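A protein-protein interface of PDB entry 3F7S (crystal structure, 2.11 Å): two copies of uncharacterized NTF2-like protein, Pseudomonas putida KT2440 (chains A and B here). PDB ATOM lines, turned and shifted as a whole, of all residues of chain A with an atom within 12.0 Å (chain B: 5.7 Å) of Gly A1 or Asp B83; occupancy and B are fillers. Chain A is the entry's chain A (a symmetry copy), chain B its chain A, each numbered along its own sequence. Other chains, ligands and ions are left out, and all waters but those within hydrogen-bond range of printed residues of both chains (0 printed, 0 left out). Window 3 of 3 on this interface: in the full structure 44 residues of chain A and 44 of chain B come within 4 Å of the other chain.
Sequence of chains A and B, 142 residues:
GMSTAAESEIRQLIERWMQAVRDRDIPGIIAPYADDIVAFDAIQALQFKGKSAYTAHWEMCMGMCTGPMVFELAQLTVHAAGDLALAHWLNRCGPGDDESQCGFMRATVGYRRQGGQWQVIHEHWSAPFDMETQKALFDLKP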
ATOM      1  N   GLY A   1     -17.014   4.128  26.490  1.00  0.00           N
ATOM      2  CA  GLY A   1     -16.940   2.833  27.247  1.00  0.00           C
ATOM      3  C   GLY A   1     -17.626   1.667  26.537  1.00  0.00           C
ATOM      4  O   GLY A   1     -17.700   1.616  25.306  1.00  0.00           O
ATOM      5  N   MET A   2     -18.160   0.745  27.324  1.00  0.00           N
ATOM      6  CA  MET A   2     -18.674  -0.491  26.792  1.00  0.00           C
ATOM      7  C   MET A   2     -20.080  -0.257  26.259  1.00  0.00           C
ATOM      8  O   MET A   2     -20.750   0.701  26.655  1.00  0.00           O
ATOM      9  CB  MET A   2     -18.659  -1.559  27.890  1.00  0.00           C
ATOM     10  CG  MET A   2     -17.279  -1.737  28.549  1.00  0.00           C
ATOM     11  SD  MET A   2     -15.883  -2.354  27.301  1.00  0.00           S
ATOM     12  CE  MET A   2     -14.581  -0.955  27.521  1.00  0.00           C
ATOM     13  N   SER A   3     -20.525  -1.123  25.367  1.00  0.00           N
ATOM     14  CA  SER A   3     -21.848  -1.029  24.763  1.00  0.00           C
ATOM     15  C   SER A   3     -22.711  -2.173  25.269  1.00  0.00           C
ATOM     16  O   SER A   3     -22.434  -3.350  24.987  1.00  0.00           O
ATOM     17  CB  SER A   3     -21.706  -1.125  23.242  1.00  0.00           C
ATOM     18  OG  SER A   3     -22.977  -1.262  22.631  1.00  0.00           O
ATOM     19  N   THR A   4     -23.760  -1.854  26.028  1.00  0.00           N
ATOM     20  CA  THR A   4     -24.648  -2.887  26.556  1.00  0.00           C
ATOM     21  C   THR A   4     -25.445  -3.534  25.415  1.00  0.00           C
ATOM     22  O   THR A   4     -25.747  -4.718  25.441  1.00  0.00           O
ATOM     23  CB  THR A   4     -25.550  -2.327  27.695  1.00  0.00           C
ATOM     24  OG1 THR A   4     -26.089  -1.092  27.279  1.00  0.00           O
ATOM     25  CG2 THR A   4     -24.734  -2.032  28.976  1.00  0.00           C
ATOM     26  N   ALA A   5     -25.755  -2.790  24.372  1.00  0.00           N
ATOM     27  CA  ALA A   5     -26.445  -3.403  23.245  1.00  0.00           C
ATOM     28  C   ALA A   5     -25.549  -4.468  22.602  1.00  0.00           C
ATOM     29  O   ALA A   5     -26.021  -5.564  22.320  1.00  0.00           O
ATOM     30  CB  ALA A   5     -26.902  -2.326  22.207  1.00  0.00           C
ATOM     31  N   ALA A   6     -24.259  -4.157  22.392  1.00  0.00           N
ATOM     32  CA  ALA A   6     -23.322  -5.106  21.747  1.00  0.00           C
ATOM     33  C   ALA A   6     -23.121  -6.323  22.634  1.00  0.00           C
ATOM     34  O   ALA A   6     -23.158  -7.446  22.175  1.00  0.00           O
ATOM     35  CB  ALA A   6     -21.955  -4.419  21.435  1.00  0.00           C
ATOM     36  N   GLU A   7     -22.942  -6.091  23.923  1.00  0.00           N
ATOM     37  CA  GLU A   7     -22.765  -7.175  24.871  1.00  0.00           C
ATOM     38  C   GLU A   7     -24.001  -8.073  24.943  1.00  0.00           C
ATOM     39  O   GLU A   7     -23.876  -9.294  25.067  1.00  0.00           O
ATOM     40  CB  GLU A   7     -22.414  -6.613  26.260  1.00  0.00           C
ATOM     41  CG  GLU A   7     -20.997  -6.046  26.309  1.00  0.00           C
ATOM     42  CD  GLU A   7     -20.704  -5.230  27.563  1.00  0.00           C
ATOM     43  OE1 GLU A   7     -21.573  -5.135  28.450  1.00  0.00           O
ATOM     44  OE2 GLU A   7     -19.594  -4.686  27.675  1.00  0.00           O
ATOM     45  N   SER A   8     -25.196  -7.488  24.888  1.00  0.00           N
ATOM     46  CA  SER A   8     -26.411  -8.315  24.790  1.00  0.00           C
ATOM     47  C   SER A   8     -26.364  -9.168  23.510  1.00  0.00           C
ATOM     48  O   SER A   8     -26.715 -10.359  23.530  1.00  0.00           O
ATOM     49  CB  SER A   8     -27.656  -7.443  24.812  1.00  0.00           C
ATOM     50  OG  SER A   8     -28.878  -8.176  24.682  1.00  0.00           O
ATOM     51  N   VAL A  78     -18.457 -10.891  29.496  1.00  0.00           N
ATOM     52  CA  VAL A  78     -18.542 -10.341  28.161  1.00  0.00           C
ATOM     53  C   VAL A  78     -18.266  -8.840  28.213  1.00  0.00           C
ATOM     54  O   VAL A  78     -18.847  -8.132  29.041  1.00  0.00           O
ATOM     55  CB  VAL A  78     -19.928 -10.585  27.506  1.00  0.00           C
ATOM     56  CG1 VAL A  78     -19.923 -10.002  26.112  1.00  0.00           C
ATOM     57  CG2 VAL A  78     -20.246 -12.061  27.467  1.00  0.00           C
ATOM     58  N   HIS A  79     -17.334  -8.367  27.372  1.00  0.00           N
ATOM     59  CA  HIS A  79     -17.080  -6.929  27.208  1.00  0.00           C
ATOM     60  C   HIS A  79     -17.107  -6.573  25.764  1.00  0.00           C
ATOM     61  O   HIS A  79     -16.517  -7.278  24.983  1.00  0.00           O
ATOM     62  CB  HIS A  79     -15.704  -6.554  27.728  1.00  0.00           C
ATOM     63  CG  HIS A  79     -15.482  -6.905  29.154  1.00  0.00           C
ATOM     64  ND1 HIS A  79     -16.213  -6.333  30.179  1.00  0.00           N
ATOM     65  CD2 HIS A  79     -14.580  -7.730  29.739  1.00  0.00           C
ATOM     66  CE1 HIS A  79     -15.784  -6.815  31.332  1.00  0.00           C
ATOM     67  NE2 HIS A  79     -14.796  -7.658  31.091  1.00  0.00           N
ATOM     68  N   ALA A  80     -17.748  -5.467  25.403  1.00  0.00           N
ATOM     69  CA  ALA A  80     -17.836  -5.044  24.003  1.00  0.00           C
ATOM     70  C   ALA A  80     -17.822  -3.518  23.889  1.00  0.00           C
ATOM     71  O   ALA A  80     -18.426  -2.821  24.697  1.00  0.00           O
ATOM     72  CB  ALA A  80     -19.087  -5.641  23.346  1.00  0.00           C
ATOM     73  N   ALA A  81     -17.073  -3.011  22.919  1.00  0.00           N
ATOM     74  CA  ALA A  81     -16.922  -1.591  22.659  1.00  0.00           C
ATOM     75  C   ALA A  81     -16.695  -1.401  21.166  1.00  0.00           C
ATOM     76  O   ALA A  81     -15.682  -1.904  20.583  1.00  0.00           O
ATOM     77  CB  ALA A  81     -15.754  -1.024  23.392  1.00  0.00           C
ATOM     78  N   GLY A  82     -17.618  -0.678  20.533  1.00  0.00           N
ATOM     79  CA  GLY A  82     -17.524  -0.413  19.092  1.00  0.00           C
ATOM     80  C   GLY A  82     -17.550  -1.669  18.252  1.00  0.00           C
ATOM     81  O   GLY A  82     -18.547  -2.379  18.214  1.00  0.00           O
ATOM     82  N   ASP A  83     -16.435  -1.957  17.599  1.00  0.00           N
ATOM     83  CA  ASP A  83     -16.373  -3.078  16.661  1.00  0.00           C
ATOM     84  C   ASP A  83     -15.636  -4.304  17.204  1.00  0.00           C
ATOM     85  O   ASP A  83     -15.425  -5.255  16.465  1.00  0.00           O
ATOM     86  CB  ASP A  83     -15.699  -2.626  15.360  1.00  0.00           C
ATOM     87  CG  ASP A  83     -16.561  -1.641  14.533  1.00  0.00           C
ATOM     88  OD1 ASP A  83     -17.791  -1.537  14.738  1.00  0.00           O
ATOM     89  OD2 ASP A  83     -15.980  -0.981  13.637  1.00  0.00           O
ATOM     90  N   LEU A  84     -15.256  -4.274  18.475  1.00  0.00           N
ATOM     91  CA  LEU A  84     -14.509  -5.357  19.086  1.00  0.00           C
ATOM     92  C   LEU A  84     -15.217  -5.853  20.347  1.00  0.00           C
ATOM     93  O   LEU A  84     -15.854  -5.075  21.039  1.00  0.00           O
ATOM     94  CB  LEU A  84     -13.121  -4.830  19.422  1.00  0.00           C
ATOM     95  CG  LEU A  84     -12.079  -5.868  19.757  1.00  0.00           C
ATOM     96  CD1 LEU A  84     -11.791  -6.771  18.531  1.00  0.00           C
ATOM     97  CD2 LEU A  84     -10.822  -5.107  20.178  1.00  0.00           C
ATOM     98  N   ALA A  85     -15.176  -7.160  20.600  1.00  0.00           N
ATOM     99  CA  ALA A  85     -15.681  -7.724  21.827  1.00  0.00           C
ATOM    100  C   ALA A  85     -14.803  -8.887  22.269  1.00  0.00           C
ATOM    101  O   ALA A  85     -14.111  -9.530  21.458  1.00  0.00           O
ATOM    102  CB  ALA A  85     -17.143  -8.203  21.677  1.00  0.00           C
ATOM    103  N   LEU A  86     -14.866  -9.150  23.565  1.00  0.00           N
ATOM    104  CA  LEU A  86     -14.132 -10.204  24.219  1.00  0.00           C
ATOM    105  C   LEU A  86     -15.091 -10.966  25.165  1.00  0.00           C
ATOM    106  O   LEU A  86     -15.832 -10.336  25.915  1.00  0.00           O
ATOM    107  CB  LEU A  86     -13.027  -9.545  25.070  1.00  0.00           C
ATOM    108  CG  LEU A  86     -12.330 -10.516  26.017  1.00  0.00           C
ATOM    109  CD1 LEU A  86     -11.337 -11.353  25.149  1.00  0.00           C
ATOM    110  CD2 LEU A  86     -11.668  -9.794  27.168  1.00  0.00           C
ATOM    111  N   TYR A 111     -14.239 -11.257  19.222  1.00  0.00           N
ATOM    112  CA  TYR A 111     -15.271 -10.985  18.223  1.00  0.00           C
ATOM    113  C   TYR A 111     -14.996  -9.637  17.564  1.00  0.00           C
ATOM    114  O   TYR A 111     -14.381  -8.749  18.170  1.00  0.00           O
ATOM    115  CB  TYR A 111     -16.683 -10.946  18.844  1.00  0.00           C
ATOM    116  CG  TYR A 111     -17.077 -12.147  19.700  1.00  0.00           C
ATOM    117  CD1 TYR A 111     -16.692 -12.213  21.021  1.00  0.00           C
ATOM    118  CD2 TYR A 111     -17.873 -13.193  19.182  1.00  0.00           C
ATOM    119  CE1 TYR A 111     -17.055 -13.275  21.823  1.00  0.00           C
ATOM    120  CE2 TYR A 111     -18.215 -14.288  19.974  1.00  0.00           C
ATOM    121  CZ  TYR A 111     -17.779 -14.322  21.286  1.00  0.00           C
ATOM    122  OH  TYR A 111     -18.083 -15.362  22.126  1.00  0.00           O
ATOM    123  N   ARG A 113     -17.011  -6.721  14.753  1.00  0.00           N
ATOM    124  CA  ARG A 113     -18.229  -6.343  14.003  1.00  0.00           C
ATOM    125  C   ARG A 113     -17.815  -5.966  12.591  1.00  0.00           C
ATOM    126  O   ARG A 113     -17.038  -5.026  12.375  1.00  0.00           O
ATOM    127  CB  ARG A 113     -19.044  -5.218  14.667  1.00  0.00           C
ATOM    128  CG  ARG A 113     -20.543  -5.185  14.212  1.00  0.00           C
ATOM    129  CD  ARG A 113     -21.320  -3.939  14.590  1.00  0.00           C
ATOM    130  NE  ARG A 113     -20.789  -3.233  15.754  1.00  0.00           N
ATOM    131  N   TRP A 118     -21.572  -9.385  14.053  1.00  0.00           N
ATOM    132  CA  TRP A 118     -20.491  -9.833  14.910  1.00  0.00           C
ATOM    133  C   TRP A 118     -20.051 -11.178  14.387  1.00  0.00           C
ATOM    134  O   TRP A 118     -20.889 -12.047  14.141  1.00  0.00           O
ATOM    135  CB  TRP A 118     -20.939  -9.945  16.361  1.00  0.00           C
ATOM    136  CG  TRP A 118     -21.152  -8.624  16.987  1.00  0.00           C
ATOM    137  CD1 TRP A 118     -22.344  -7.978  17.151  1.00  0.00           C
ATOM    138  CD2 TRP A 118     -20.153  -7.764  17.540  1.00  0.00           C
ATOM    139  NE1 TRP A 118     -22.154  -6.768  17.759  1.00  0.00           N
ATOM    140  CE2 TRP A 118     -20.818  -6.603  18.013  1.00  0.00           C
ATOM    141  CE3 TRP A 118     -18.767  -7.836  17.647  1.00  0.00           C
ATOM    142  CZ2 TRP A 118     -20.143  -5.535  18.606  1.00  0.00           C
ATOM    143  CZ3 TRP A 118     -18.084  -6.779  18.263  1.00  0.00           C
ATOM    144  CH2 TRP A 118     -18.778  -5.637  18.720  1.00  0.00           C
ATOM    145  N   ALA B  81     -10.093  -1.168  19.497  1.00  0.00           N
ATOM    146  CA  ALA B  81     -11.171  -0.275  19.113  1.00  0.00           C
ATOM    147  C   ALA B  81     -11.731   0.367  20.375  1.00  0.00           C
ATOM    148  O   ALA B  81     -12.261  -0.336  21.293  1.00  0.00           O
ATOM    149  CB  ALA B  81     -12.270  -1.011  18.427  1.00  0.00           C
ATOM    150  N   GLY B  82     -11.629   1.694  20.437  1.00  0.00           N
ATOM    151  CA  GLY B  82     -12.130   2.444  21.594  1.00  0.00           C
ATOM    152  C   GLY B  82     -11.449   2.065  22.890  1.00  0.00           C
ATOM    153  O   GLY B  82     -10.257   2.291  23.063  1.00  0.00           O
ATOM    154  N   ASP B  83     -12.206   1.460  23.792  1.00  0.00           N
ATOM    155  CA  ASP B  83     -11.696   1.152  25.128  1.00  0.00           C
ATOM    156  C   ASP B  83     -11.350  -0.323  25.337  1.00  0.00           C
ATOM    157  O   ASP B  83     -11.025  -0.713  26.449  1.00  0.00           O
ATOM    158  CB  ASP B  83     -12.722   1.579  26.184  1.00  0.00           C
ATOM    159  CG  ASP B  83     -12.870   3.116  26.309  1.00  0.00           C
ATOM    160  OD1 ASP B  83     -11.988   3.884  25.861  1.00  0.00           O
ATOM    161  OD2 ASP B  83     -13.888   3.549  26.900  1.00  0.00           O
ATOM    162  N   LEU B  84     -11.422  -1.123  24.280  1.00  0.00           N
ATOM    163  CA  LEU B  84     -11.165  -2.548  24.367  1.00  0.00           C
ATOM    164  C   LEU B  84     -10.093  -2.963  23.359  1.00  0.00           C
ATOM    165  O   LEU B  84     -10.000  -2.382  22.289  1.00  0.00           O
ATOM    166  CB  LEU B  84     -12.474  -3.273  24.086  1.00  0.00           C
ATOM    167  CG  LEU B  84     -12.514  -4.736  24.448  1.00  0.00           C
ATOM    168  CD1 LEU B  84     -12.364  -4.927  25.978  1.00  0.00           C
ATOM    169  CD2 LEU B  84     -13.862  -5.271  23.964  1.00  0.00           C
ATOM    170  N   ALA B  85      -9.232  -3.907  23.733  1.00  0.00           N
ATOM    171  CA  ALA B  85      -8.272  -4.480  22.823  1.00  0.00           C
ATOM    172  C   ALA B  85      -8.090  -5.962  23.118  1.00  0.00           C
ATOM    173  O   ALA B  85      -8.333  -6.441  24.241  1.00  0.00           O
ATOM    174  CB  ALA B  85      -6.905  -3.761  22.906  1.00  0.00           C
ATOM    175  N   TYR B 111      -7.524  -6.416  26.951  1.00  0.00           N
ATOM    176  CA  TYR B 111      -7.114  -5.132  27.516  1.00  0.00           C
ATOM    177  C   TYR B 111      -8.310  -4.183  27.536  1.00  0.00           C
ATOM    178  O   TYR B 111      -9.231  -4.306  26.717  1.00  0.00           O
ATOM    179  CB  TYR B 111      -5.982  -4.473  26.701  1.00  0.00           C
ATOM    180  CG  TYR B 111      -4.759  -5.343  26.422  1.00  0.00           C
ATOM    181  CD1 TYR B 111      -4.764  -6.227  25.365  1.00  0.00           C
ATOM    182  CD2 TYR B 111      -3.586  -5.239  27.202  1.00  0.00           C
ATOM    183  CE1 TYR B 111      -3.663  -7.006  25.075  1.00  0.00           C
ATOM    184  CE2 TYR B 111      -2.481  -6.048  26.940  1.00  0.00           C
ATOM    185  CZ  TYR B 111      -2.546  -6.941  25.886  1.00  0.00           C
ATOM    186  OH  TYR B 111      -1.496  -7.762  25.564  1.00  0.00           O
ATOM    187  N   ARG B 112      -8.293  -3.261  28.480  1.00  0.00           N
ATOM    188  CA  ARG B 112      -9.320  -2.224  28.619  1.00  0.00           C
ATOM    189  C   ARG B 112      -8.728  -0.875  28.979  1.00  0.00           C
ATOM    190  O   ARG B 112      -7.840  -0.791  29.855  1.00  0.00           O
ATOM    191  CB  ARG B 112     -10.275  -2.601  29.728  1.00  0.00           C
ATOM    192  CG  ARG B 112     -11.416  -1.610  29.908  1.00  0.00           C
ATOM    193  CD  ARG B 112     -12.532  -2.213  30.752  1.00  0.00           C
ATOM    194  NE  ARG B 112     -13.609  -1.229  30.905  1.00  0.00           N
ATOM    195  CZ  ARG B 112     -14.816  -1.474  31.422  1.00  0.00           C
ATOM    196  NH1 ARG B 112     -15.141  -2.699  31.847  1.00  0.00           N
ATOM    197  NH2 ARG B 112     -15.706  -0.483  31.499  1.00  0.00           N
ATOM    198  N   ARG B 113      -9.210   0.180  28.321  1.00  0.00           N
ATOM    199  CA  ARG B 113      -8.687   1.538  28.587  1.00  0.00           C
ATOM    200  C   ARG B 113      -9.492   2.138  29.727  1.00  0.00           C
ATOM    201  O   ARG B 113     -10.714   2.311  29.633  1.00  0.00           O
ATOM    202  CB  ARG B 113      -8.692   2.460  27.353  1.00  0.00           C
ATOM    203  CG  ARG B 113      -7.684   3.655  27.466  1.00  0.00           C
ATOM    204  CD  ARG B 113      -7.846   4.755  26.436  1.00  0.00           C
ATOM    205  NE  ARG B 113      -8.486   4.322  25.195  1.00  0.00           N
ATOM    206  N   TRP B 118      -4.233   1.807  29.309  1.00  0.00           N
ATOM    207  CA  TRP B 118      -4.589   0.445  28.956  1.00  0.00           C
ATOM    208  C   TRP B 118      -4.139  -0.432  30.098  1.00  0.00           C
ATOM    209  O   TRP B 118      -3.001  -0.314  30.553  1.00  0.00           O
ATOM    210  CB  TRP B 118      -3.924   0.014  27.656  1.00  0.00           C
ATOM    211  CG  TRP B 118      -4.507   0.683  26.476  1.00  0.00           C
ATOM    212  CD1 TRP B 118      -4.013   1.778  25.827  1.00  0.00           C
ATOM    213  CD2 TRP B 118      -5.705   0.318  25.785  1.00  0.00           C
ATOM    214  NE1 TRP B 118      -4.828   2.127  24.786  1.00  0.00           N
ATOM    215  CE2 TRP B 118      -5.878   1.250  24.730  1.00  0.00           C
ATOM    216  CE3 TRP B 118      -6.666  -0.672  25.974  1.00  0.00           C
ATOM    217  CZ2 TRP B 118      -6.962   1.204  23.853  1.00  0.00           C
ATOM    218  CZ3 TRP B 118      -7.744  -0.740  25.083  1.00  0.00           C
ATOM    219  CH2 TRP B 118      -7.887   0.207  24.044  1.00  0.00           C
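The side-chain carboxylate (OD2) of Asp B83 sits close to the backbone NH (N) of Gly A1 (3.2 Å).
Ala A81 touches its own counterpart, Ala B81.
Leu B84 touches its own counterpart, Leu A84.
Leu A84 touches Ala B85, and with the chains exchanged Ala A85 touches Leu B84.
Positions printed for both chains: 81, 82, 83, 84, 85, 111, 113 and 118.
Of the 9 pairs that touch across the chains among the printed residues, 4 have their exchanged pair printed and touching as well.
Among the printed residues, pairs that only touch across the chains: Met A2 with Asp B83 (3.4 Å), His A79 with Leu B84 (3.5 Å), Met A2 with Arg B112 (3.5 Å), Leu A84 with Leu B84 (3.5 Å), Leu A84 with Ala B85 (3.7 Å), Ala A85 with Leu B84 (3.7 Å), Ala A81 with Ala B81 (3.8 Å) and Ala A80 with Leu B84 (3.98 Å).
OE2 of Glu A7 lies within hydrogen-bond range of N of Ala A80.
O of Ala A85 is in hydrogen-bond range of N of Tyr A111, 2.8 Å away.
The side-chain carboxylate (OD1) of Asp B83 lies within salt-bridge range of the guanidinium group (NE) of Arg B113 (3.6 Å).
The backbone carbonyl oxygen of Ala B85 is in hydrogen-bond range of the backbone NH of Tyr B111 (2.8 Å).
N of Ser A3 is in hydrogen-bond range of O of Ala A80 (2.8 Å).
The backbone carbonyl oxygen (O) of His A79 lies within hydrogen-bond range of the backbone NH (N) of Leu A86.
Ser A8 touches none of the printed residues of chain B.
Of the printed residues of chain B, Ala A80 touches Leu B84 (3.98 Å).
No residue of chain A comes within 4 Å of Gly B82.
Asp B83 touches just these residues of chain A: Gly A1 (3.2 Å) and Met A2 (3.4 Å).
Of the printed residues of chain A, Leu B84 touches His A79, Ala A80, Leu A84 and Ala A85.
No residue of chain A comes within 4 Å of Arg B113.
The nearest printed residue of chain B that does not touch Ala A81 is Leu B84 (4.04 Å).
Of the 9 printed residues of chain B, 5 touch a printed residue of chain A.
Hydrophobic or aromatic side chains of chain B that line the printed part of chain A: Leu B84.
Hydrophobic or aromatic side chains of chain A that line the printed part of chain B: Met A2 and Leu A84.
Along chain A the printed residues that touch a printed residue of chain B span positions 1 to 85.
Among the printed residues, no Asp or Glu carboxylate lies within 4 Å of a Lys or Arg side-chain nitrogen of the other chain.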
